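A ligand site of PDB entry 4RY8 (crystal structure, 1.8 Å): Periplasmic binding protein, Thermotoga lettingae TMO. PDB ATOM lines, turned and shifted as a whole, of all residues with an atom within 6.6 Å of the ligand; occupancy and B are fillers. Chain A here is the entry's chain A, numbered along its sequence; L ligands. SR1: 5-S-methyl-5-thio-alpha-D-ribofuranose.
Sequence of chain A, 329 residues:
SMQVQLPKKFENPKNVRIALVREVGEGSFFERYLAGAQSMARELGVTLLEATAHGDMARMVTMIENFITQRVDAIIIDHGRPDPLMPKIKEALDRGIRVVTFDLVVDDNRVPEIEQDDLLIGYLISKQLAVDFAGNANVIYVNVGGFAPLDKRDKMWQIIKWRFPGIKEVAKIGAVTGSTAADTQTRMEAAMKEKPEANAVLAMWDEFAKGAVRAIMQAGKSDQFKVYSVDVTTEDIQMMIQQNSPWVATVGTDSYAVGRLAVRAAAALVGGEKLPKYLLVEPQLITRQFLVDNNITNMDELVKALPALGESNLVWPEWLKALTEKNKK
The backbone NH (N) of His 79 lies within hydrogen-bond range of the backbone carbonyl oxygen (O) of Phe 102, at 2.9 Å.
The side-chain carboxylate (OD2) of Asp 103 sits close to a ring nitrogen (NE2) of His 79, at 3.3 Å.
NH2 of Arg 153 is in salt-bridge range of OD1 of Asp 118, 2.6 Å away.
The side-chain hydroxyl (OG1) of Thr 253 lies within hydrogen-bond range of the side-chain amide oxygen (OE1) of Gln 116 (2.4 Å).
The side-chain carboxylate of Asp 231 lies within hydrogen-bond range of the backbone NH of Asp 206 (3.1 Å).
The guanidinium group of Arg 153 lies close to the side-chain amide nitrogen of Gln 116 (3.5 Å).
The guanidinium group (NH1) of Arg 153 is in hydrogen-bond range of the backbone carbonyl oxygen (O) of Met 204.
Residues that only touch the ligand: Phe 29 (3.5 Å), Phe 30 (3.7 Å), Phe 147 (3.7 Å), Pro 149 (3.6 Å), Leu 150 (3.999 Å), Met 204 (3.7 Å) and Trp 205 (3.3 Å).
12 residues have an atom within 4 Å of the ligand: Phe 29, Phe 30, His 79, Asp 103, Gln 116, Phe 147, Pro 149, Leu 150, Arg 153, Met 204, Trp 205 and Asp 231.
Along chain A the residues within 4 Å of the ligand span positions 29 to 231.
The nearest printed residue that does not touch the ligand is Val 176 (4.03 Å).
An oxygen (O1) of the ligand is in hydrogen-bond range of the side-chain carboxylate (OD2) of Asp 103 (2.4 Å).
The side-chain amide nitrogen of Gln 116 lies within hydrogen-bond range of an oxygen (O2) of the ligand (2.9 Å).
The guanidinium group (NH1) of Arg 153 is in hydrogen-bond range of an oxygen (O3) of the ligand (2.9 Å).
A ring nitrogen (NE2) of His 79 is in hydrogen-bond range of an oxygen (O4) of the ligand, 2.9 Å away.
OD1 of Asp 231 is in hydrogen-bond range of O2 of the ligand, at 2.6 Å.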
ATOM      1  N   VAL A  24     -20.012  11.384 -25.105  1.00  0.00           N
ATOM      2  CA  VAL A  24     -20.010  12.446 -24.097  1.00  0.00           C
ATOM      3  C   VAL A  24     -21.394  13.045 -24.079  1.00  0.00           C
ATOM      4  O   VAL A  24     -22.010  13.261 -25.144  1.00  0.00           O
ATOM      5  CB  VAL A  24     -18.965  13.554 -24.440  1.00  0.00           C
ATOM      6  CG1 VAL A  24     -18.984  14.687 -23.407  1.00  0.00           C
ATOM      7  CG2 VAL A  24     -17.586  12.967 -24.497  1.00  0.00           C
ATOM      8  N   PHE A  29     -24.229  22.268 -24.158  1.00  0.00           N
ATOM      9  CA  PHE A  29     -24.054  22.045 -25.601  1.00  0.00           C
ATOM     10  C   PHE A  29     -24.604  20.682 -26.003  1.00  0.00           C
ATOM     11  O   PHE A  29     -25.455  20.588 -26.883  1.00  0.00           O
ATOM     12  CB  PHE A  29     -22.597  22.203 -26.082  1.00  0.00           C
ATOM     13  CG  PHE A  29     -22.401  21.783 -27.531  1.00  0.00           C
ATOM     14  CD1 PHE A  29     -22.342  20.434 -27.899  1.00  0.00           C
ATOM     15  CD2 PHE A  29     -22.262  22.732 -28.521  1.00  0.00           C
ATOM     16  CE1 PHE A  29     -22.176  20.055 -29.220  1.00  0.00           C
ATOM     17  CE2 PHE A  29     -22.054  22.350 -29.826  1.00  0.00           C
ATOM     18  CZ  PHE A  29     -22.020  21.026 -30.179  1.00  0.00           C
ATOM     19  N   PHE A  30     -24.154  19.630 -25.327  1.00  0.00           N
ATOM     20  CA  PHE A  30     -24.629  18.299 -25.615  1.00  0.00           C
ATOM     21  C   PHE A  30     -26.104  18.100 -25.256  1.00  0.00           C
ATOM     22  O   PHE A  30     -26.782  17.389 -25.985  1.00  0.00           O
ATOM     23  CB  PHE A  30     -23.770  17.257 -24.944  1.00  0.00           C
ATOM     24  CG  PHE A  30     -22.385  17.203 -25.529  1.00  0.00           C
ATOM     25  CD1 PHE A  30     -22.208  16.858 -26.858  1.00  0.00           C
ATOM     26  CD2 PHE A  30     -21.282  17.492 -24.761  1.00  0.00           C
ATOM     27  CE1 PHE A  30     -20.941  16.803 -27.416  1.00  0.00           C
ATOM     28  CE2 PHE A  30     -20.028  17.428 -25.291  1.00  0.00           C
ATOM     29  CZ  PHE A  30     -19.840  17.084 -26.612  1.00  0.00           C
ATOM     30  N   HIS A  79     -19.021  11.629 -31.514  1.00  0.00           N
ATOM     31  CA  HIS A  79     -17.702  11.595 -30.925  1.00  0.00           C
ATOM     32  C   HIS A  79     -17.179  10.194 -30.962  1.00  0.00           C
ATOM     33  O   HIS A  79     -17.611   9.432 -31.825  1.00  0.00           O
ATOM     34  CB  HIS A  79     -17.697  12.225 -29.543  1.00  0.00           C
ATOM     35  CG  HIS A  79     -17.904  13.695 -29.565  1.00  0.00           C
ATOM     36  ND1 HIS A  79     -19.117  14.265 -29.900  1.00  0.00           N
ATOM     37  CD2 HIS A  79     -17.073  14.707 -29.239  1.00  0.00           C
ATOM     38  CE1 HIS A  79     -19.005  15.573 -29.820  1.00  0.00           C
ATOM     39  NE2 HIS A  79     -17.791  15.871 -29.408  1.00  0.00           N
ATOM     40  N   PHE A 102     -21.208  12.422 -36.211  1.00  0.00           N
ATOM     41  CA  PHE A 102     -20.964  13.753 -35.789  1.00  0.00           C
ATOM     42  C   PHE A 102     -19.636  13.681 -34.999  1.00  0.00           C
ATOM     43  O   PHE A 102     -19.521  12.884 -34.096  1.00  0.00           O
ATOM     44  CB  PHE A 102     -22.072  14.273 -34.888  1.00  0.00           C
ATOM     45  CG  PHE A 102     -21.781  15.619 -34.283  1.00  0.00           C
ATOM     46  CD1 PHE A 102     -21.529  16.724 -35.091  1.00  0.00           C
ATOM     47  CD2 PHE A 102     -21.864  15.811 -32.942  1.00  0.00           C
ATOM     48  CE1 PHE A 102     -21.252  17.946 -34.550  1.00  0.00           C
ATOM     49  CE2 PHE A 102     -21.637  17.063 -32.370  1.00  0.00           C
ATOM     50  CZ  PHE A 102     -21.319  18.128 -33.204  1.00  0.00           C
ATOM     51  N   ASP A 103     -18.690  14.519 -35.395  1.00  0.00           N
ATOM     52  CA  ASP A 103     -17.439  14.648 -34.654  1.00  0.00           C
ATOM     53  C   ASP A 103     -16.653  13.354 -34.597  1.00  0.00           C
ATOM     54  O   ASP A 103     -16.074  12.988 -33.576  1.00  0.00           O
ATOM     55  CB  ASP A 103     -17.695  15.243 -33.292  1.00  0.00           C
ATOM     56  CG  ASP A 103     -17.813  16.767 -33.337  1.00  0.00           C
ATOM     57  OD1 ASP A 103     -17.632  17.342 -34.428  1.00  0.00           O
ATOM     58  OD2 ASP A 103     -18.022  17.409 -32.274  1.00  0.00           O
ATOM     59  N   GLN A 116     -18.939  20.983 -37.233  1.00  0.00           N
ATOM     60  CA  GLN A 116     -19.194  22.391 -37.222  1.00  0.00           C
ATOM     61  C   GLN A 116     -18.166  23.271 -37.968  1.00  0.00           C
ATOM     62  O   GLN A 116     -18.001  24.437 -37.646  1.00  0.00           O
ATOM     63  CB  GLN A 116     -19.380  22.814 -35.807  1.00  0.00           C
ATOM     64  CG  GLN A 116     -20.380  21.996 -34.975  1.00  0.00           C
ATOM     65  CD  GLN A 116     -20.351  22.407 -33.523  1.00  0.00           C
ATOM     66  OE1 GLN A 116     -21.050  23.337 -33.086  1.00  0.00           O
ATOM     67  NE2 GLN A 116     -19.481  21.730 -32.747  1.00  0.00           N
ATOM     68  N   ASP A 118     -14.727  22.590 -37.853  1.00  0.00           N
ATOM     69  CA  ASP A 118     -13.818  22.805 -36.712  1.00  0.00           C
ATOM     70  C   ASP A 118     -12.485  23.495 -37.000  1.00  0.00           C
ATOM     71  O   ASP A 118     -11.983  24.263 -36.153  1.00  0.00           O
ATOM     72  CB  ASP A 118     -13.593  21.524 -35.929  1.00  0.00           C
ATOM     73  CG  ASP A 118     -14.809  21.119 -35.114  1.00  0.00           C
ATOM     74  OD1 ASP A 118     -15.256  21.936 -34.290  1.00  0.00           O
ATOM     75  OD2 ASP A 118     -15.333  20.036 -35.349  1.00  0.00           O
ATOM     76  N   ILE A 121     -13.405  27.033 -37.037  1.00  0.00           N
ATOM     77  CA  ILE A 121     -13.701  27.469 -35.682  1.00  0.00           C
ATOM     78  C   ILE A 121     -12.365  27.706 -35.000  1.00  0.00           C
ATOM     79  O   ILE A 121     -12.211  28.692 -34.338  1.00  0.00           O
ATOM     80  CB  ILE A 121     -14.499  26.440 -34.832  1.00  0.00           C
ATOM     81  CG1 ILE A 121     -15.951  26.333 -35.217  1.00  0.00           C
ATOM     82  CG2 ILE A 121     -14.417  26.765 -33.333  1.00  0.00           C
ATOM     83  CD1 ILE A 121     -16.698  25.280 -34.391  1.00  0.00           C
ATOM     84  N   VAL A 144      -7.706  19.516 -24.804  1.00  0.00           N
ATOM     85  CA  VAL A 144      -7.158  18.173 -24.566  1.00  0.00           C
ATOM     86  C   VAL A 144      -7.275  17.352 -25.845  1.00  0.00           C
ATOM     87  O   VAL A 144      -8.163  17.573 -26.697  1.00  0.00           O
ATOM     88  CB  VAL A 144      -7.812  17.508 -23.331  1.00  0.00           C
ATOM     89  CG1 VAL A 144      -9.226  17.031 -23.607  1.00  0.00           C
ATOM     90  CG2 VAL A 144      -6.967  16.363 -22.812  1.00  0.00           C
ATOM     91  N   PHE A 147     -10.147  14.014 -28.948  1.00  0.00           N
ATOM     92  CA  PHE A 147     -11.508  14.348 -29.436  1.00  0.00           C
ATOM     93  C   PHE A 147     -11.363  15.045 -30.784  1.00  0.00           C
ATOM     94  O   PHE A 147     -10.627  16.032 -30.896  1.00  0.00           O
ATOM     95  CB  PHE A 147     -12.206  15.259 -28.446  1.00  0.00           C
ATOM     96  CG  PHE A 147     -12.578  14.565 -27.151  1.00  0.00           C
ATOM     97  CD1 PHE A 147     -13.819  13.930 -26.987  1.00  0.00           C
ATOM     98  CD2 PHE A 147     -11.676  14.570 -26.078  1.00  0.00           C
ATOM     99  CE1 PHE A 147     -14.148  13.303 -25.784  1.00  0.00           C
ATOM    100  CE2 PHE A 147     -11.989  13.933 -24.871  1.00  0.00           C
ATOM    101  CZ  PHE A 147     -13.219  13.291 -24.718  1.00  0.00           C
ATOM    102  N   ALA A 148     -12.079  14.527 -31.778  1.00  0.00           N
ATOM    103  CA  ALA A 148     -12.009  15.022 -33.151  1.00  0.00           C
ATOM    104  C   ALA A 148     -12.120  16.527 -33.266  1.00  0.00           C
ATOM    105  O   ALA A 148     -11.281  17.163 -33.888  1.00  0.00           O
ATOM    106  CB  ALA A 148     -13.041  14.347 -34.020  1.00  0.00           C
ATOM    107  N   PRO A 149     -13.202  17.110 -32.728  1.00  0.00           N
ATOM    108  CA  PRO A 149     -13.294  18.545 -32.811  1.00  0.00           C
ATOM    109  C   PRO A 149     -12.166  19.306 -32.097  1.00  0.00           C
ATOM    110  O   PRO A 149     -11.648  20.284 -32.607  1.00  0.00           O
ATOM    111  CB  PRO A 149     -14.652  18.854 -32.122  1.00  0.00           C
ATOM    112  CG  PRO A 149     -14.944  17.673 -31.301  1.00  0.00           C
ATOM    113  CD  PRO A 149     -14.364  16.518 -32.066  1.00  0.00           C
ATOM    114  N   LEU A 150     -11.801  18.852 -30.937  1.00  0.00           N
ATOM    115  CA  LEU A 150     -10.684  19.426 -30.172  1.00  0.00           C
ATOM    116  C   LEU A 150      -9.306  19.355 -30.865  1.00  0.00           C
ATOM    117  O   LEU A 150      -8.600  20.372 -30.840  1.00  0.00           O
ATOM    118  CB  LEU A 150     -10.588  18.768 -28.815  1.00  0.00           C
ATOM    119  CG  LEU A 150     -11.880  18.831 -28.002  1.00  0.00           C
ATOM    120  CD1 LEU A 150     -11.642  18.382 -26.578  1.00  0.00           C
ATOM    121  CD2 LEU A 150     -12.515  20.229 -28.010  1.00  0.00           C
ATOM    122  N   ARG A 153      -9.425  21.882 -33.875  1.00  0.00           N
ATOM    123  CA  ARG A 153      -9.257  23.233 -33.389  1.00  0.00           C
ATOM    124  C   ARG A 153      -7.788  23.369 -32.953  1.00  0.00           C
ATOM    125  O   ARG A 153      -7.160  24.378 -33.205  1.00  0.00           O
ATOM    126  CB  ARG A 153     -10.154  23.528 -32.222  1.00  0.00           C
ATOM    127  CG  ARG A 153     -11.613  23.554 -32.671  1.00  0.00           C
ATOM    128  CD  ARG A 153     -12.587  23.279 -31.538  1.00  0.00           C
ATOM    129  NE  ARG A 153     -13.931  23.034 -32.069  1.00  0.00           N
ATOM    130  CZ  ARG A 153     -14.969  22.621 -31.348  1.00  0.00           C
ATOM    131  NH1 ARG A 153     -14.841  22.463 -30.046  1.00  0.00           N
ATOM    132  NH2 ARG A 153     -16.180  22.393 -31.926  1.00  0.00           N
ATOM    133  N   VAL A 176     -11.396  16.138 -19.846  1.00  0.00           N
ATOM    134  CA  VAL A 176     -12.817  15.817 -19.899  1.00  0.00           C
ATOM    135  C   VAL A 176     -13.136  14.737 -18.869  1.00  0.00           C
ATOM    136  O   VAL A 176     -12.765  13.596 -19.040  1.00  0.00           O
ATOM    137  CB  VAL A 176     -13.222  15.325 -21.318  1.00  0.00           C
ATOM    138  CG1 VAL A 176     -14.705  15.010 -21.400  1.00  0.00           C
ATOM    139  CG2 VAL A 176     -12.865  16.381 -22.368  1.00  0.00           C
ATOM    140  N   MET A 204     -11.228  25.567 -25.706  1.00  0.00           N
ATOM    141  CA  MET A 204     -11.847  25.036 -26.918  1.00  0.00           C
ATOM    142  C   MET A 204     -13.180  24.217 -26.762  1.00  0.00           C
ATOM    143  O   MET A 204     -13.599  23.542 -27.695  1.00  0.00           O
ATOM    144  CB  MET A 204     -10.815  24.232 -27.669  1.00  0.00           C
ATOM    145  CG  MET A 204      -9.658  25.091 -28.213  1.00  0.00           C
ATOM    146  SD  MET A 204     -10.072  26.396 -29.377  1.00  0.00           S
ATOM    147  CE  MET A 204      -8.485  26.627 -30.266  1.00  0.00           C
ATOM    148  N   TRP A 205     -13.804  24.323 -25.609  1.00  0.00           N
ATOM    149  CA  TRP A 205     -15.183  23.831 -25.362  1.00  0.00           C
ATOM    150  C   TRP A 205     -15.764  24.776 -24.316  1.00  0.00           C
ATOM    151  O   TRP A 205     -15.044  25.203 -23.421  1.00  0.00           O
ATOM    152  CB  TRP A 205     -15.094  22.378 -24.895  1.00  0.00           C
ATOM    153  CG  TRP A 205     -16.288  21.671 -24.439  1.00  0.00           C
ATOM    154  CD1 TRP A 205     -17.608  21.883 -24.827  1.00  0.00           C
ATOM    155  CD2 TRP A 205     -16.315  20.595 -23.538  1.00  0.00           C
ATOM    156  NE1 TRP A 205     -18.429  20.985 -24.219  1.00  0.00           N
ATOM    157  CE2 TRP A 205     -17.658  20.186 -23.408  1.00  0.00           C
ATOM    158  CE3 TRP A 205     -15.326  19.912 -22.809  1.00  0.00           C
ATOM    159  CZ2 TRP A 205     -18.042  19.144 -22.546  1.00  0.00           C
ATOM    160  CZ3 TRP A 205     -15.699  18.865 -22.003  1.00  0.00           C
ATOM    161  CH2 TRP A 205     -17.049  18.485 -21.870  1.00  0.00           C
ATOM    162  N   ASP A 206     -17.048  25.140 -24.422  1.00  0.00           N
ATOM    163  CA  ASP A 206     -17.625  26.102 -23.492  1.00  0.00           C
ATOM    164  C   ASP A 206     -17.593  25.600 -22.061  1.00  0.00           C
ATOM    165  O   ASP A 206     -17.615  26.404 -21.128  1.00  0.00           O
ATOM    166  CB  ASP A 206     -19.053  26.634 -23.889  1.00  0.00           C
ATOM    167  CG  ASP A 206     -20.137  25.558 -24.013  1.00  0.00           C
ATOM    168  OD1 ASP A 206     -19.819  24.390 -23.860  1.00  0.00           O
ATOM    169  OD2 ASP A 206     -21.368  25.895 -24.294  1.00  0.00           O
ATOM    170  N   PHE A 208     -15.042  23.989 -20.654  1.00  0.00           N
ATOM    171  CA  PHE A 208     -13.706  24.461 -20.233  1.00  0.00           C
ATOM    172  C   PHE A 208     -13.766  25.969 -19.889  1.00  0.00           C
ATOM    173  O   PHE A 208     -13.288  26.419 -18.849  1.00  0.00           O
ATOM    174  CB  PHE A 208     -12.651  24.282 -21.351  1.00  0.00           C
ATOM    175  CG  PHE A 208     -12.246  22.838 -21.646  1.00  0.00           C
ATOM    176  CD1 PHE A 208     -12.177  21.850 -20.662  1.00  0.00           C
ATOM    177  CD2 PHE A 208     -11.842  22.507 -22.924  1.00  0.00           C
ATOM    178  CE1 PHE A 208     -11.840  20.568 -21.001  1.00  0.00           C
ATOM    179  CE2 PHE A 208     -11.462  21.223 -23.247  1.00  0.00           C
ATOM    180  CZ  PHE A 208     -11.461  20.253 -22.285  1.00  0.00           C
ATOM    181  N   VAL A 230     -15.012  28.390 -27.521  1.00  0.00           N
ATOM    182  CA  VAL A 230     -15.853  27.784 -28.532  1.00  0.00           C
ATOM    183  C   VAL A 230     -17.182  27.366 -27.920  1.00  0.00           C
ATOM    184  O   VAL A 230     -17.243  26.988 -26.716  1.00  0.00           O
ATOM    185  CB  VAL A 230     -15.121  26.554 -29.137  1.00  0.00           C
ATOM    186  CG1 VAL A 230     -15.914  25.887 -30.248  1.00  0.00           C
ATOM    187  CG2 VAL A 230     -13.746  26.957 -29.680  1.00  0.00           C
ATOM    188  N   ASP A 231     -18.253  27.485 -28.742  1.00  0.00           N
ATOM    189  CA  ASP A 231     -19.640  27.139 -28.431  1.00  0.00           C
ATOM    190  C   ASP A 231     -20.443  28.273 -27.839  1.00  0.00           C
ATOM    191  O   ASP A 231     -19.913  29.224 -27.257  1.00  0.00           O
ATOM    192  CB  ASP A 231     -19.889  25.878 -27.551  1.00  0.00           C
ATOM    193  CG  ASP A 231     -19.017  24.678 -27.963  1.00  0.00           C
ATOM    194  OD1 ASP A 231     -19.046  24.300 -29.150  1.00  0.00           O
ATOM    195  OD2 ASP A 231     -18.333  24.089 -27.052  1.00  0.00           O
ATOM    196  N   THR A 253     -22.045  27.292 -33.119  1.00  0.00           N
ATOM    197  CA  THR A 253     -23.278  27.025 -33.850  1.00  0.00           C
ATOM    198  C   THR A 253     -24.447  26.852 -32.831  1.00  0.00           C
ATOM    199  O   THR A 253     -24.239  26.789 -31.602  1.00  0.00           O
ATOM    200  CB  THR A 253     -23.159  25.713 -34.680  1.00  0.00           C
ATOM    201  OG1 THR A 253     -23.036  24.576 -33.801  1.00  0.00           O
ATOM    202  CG2 THR A 253     -21.949  25.731 -35.625  1.00  0.00           C
HETATM  203  CS  SR1 L   1     -15.333  16.999 -25.497  1.00  0.00           C
HETATM  204  S   SR1 L   1     -15.524  17.378 -27.224  1.00  0.00           S
HETATM  205  C5  SR1 L   1     -16.432  18.887 -26.891  1.00  0.00           C
HETATM  206  C4  SR1 L   1     -16.730  19.638 -28.182  1.00  0.00           C
HETATM  207  O4  SR1 L   1     -17.456  18.726 -28.988  1.00  0.00           O
HETATM  208  C1  SR1 L   1     -18.485  19.401 -29.724  1.00  0.00           C
HETATM  209  O1  SR1 L   1     -18.011  19.471 -31.033  1.00  0.00           O
HETATM  210  C2  SR1 L   1     -18.650  20.766 -29.097  1.00  0.00           C
HETATM  211  O2  SR1 L   1     -18.432  21.872 -30.006  1.00  0.00           O
HETATM  212  C3  SR1 L   1     -17.630  20.820 -27.983  1.00  0.00           C
HETATM  213  O3  SR1 L   1     -16.938  22.027 -28.088  1.00  0.00           O
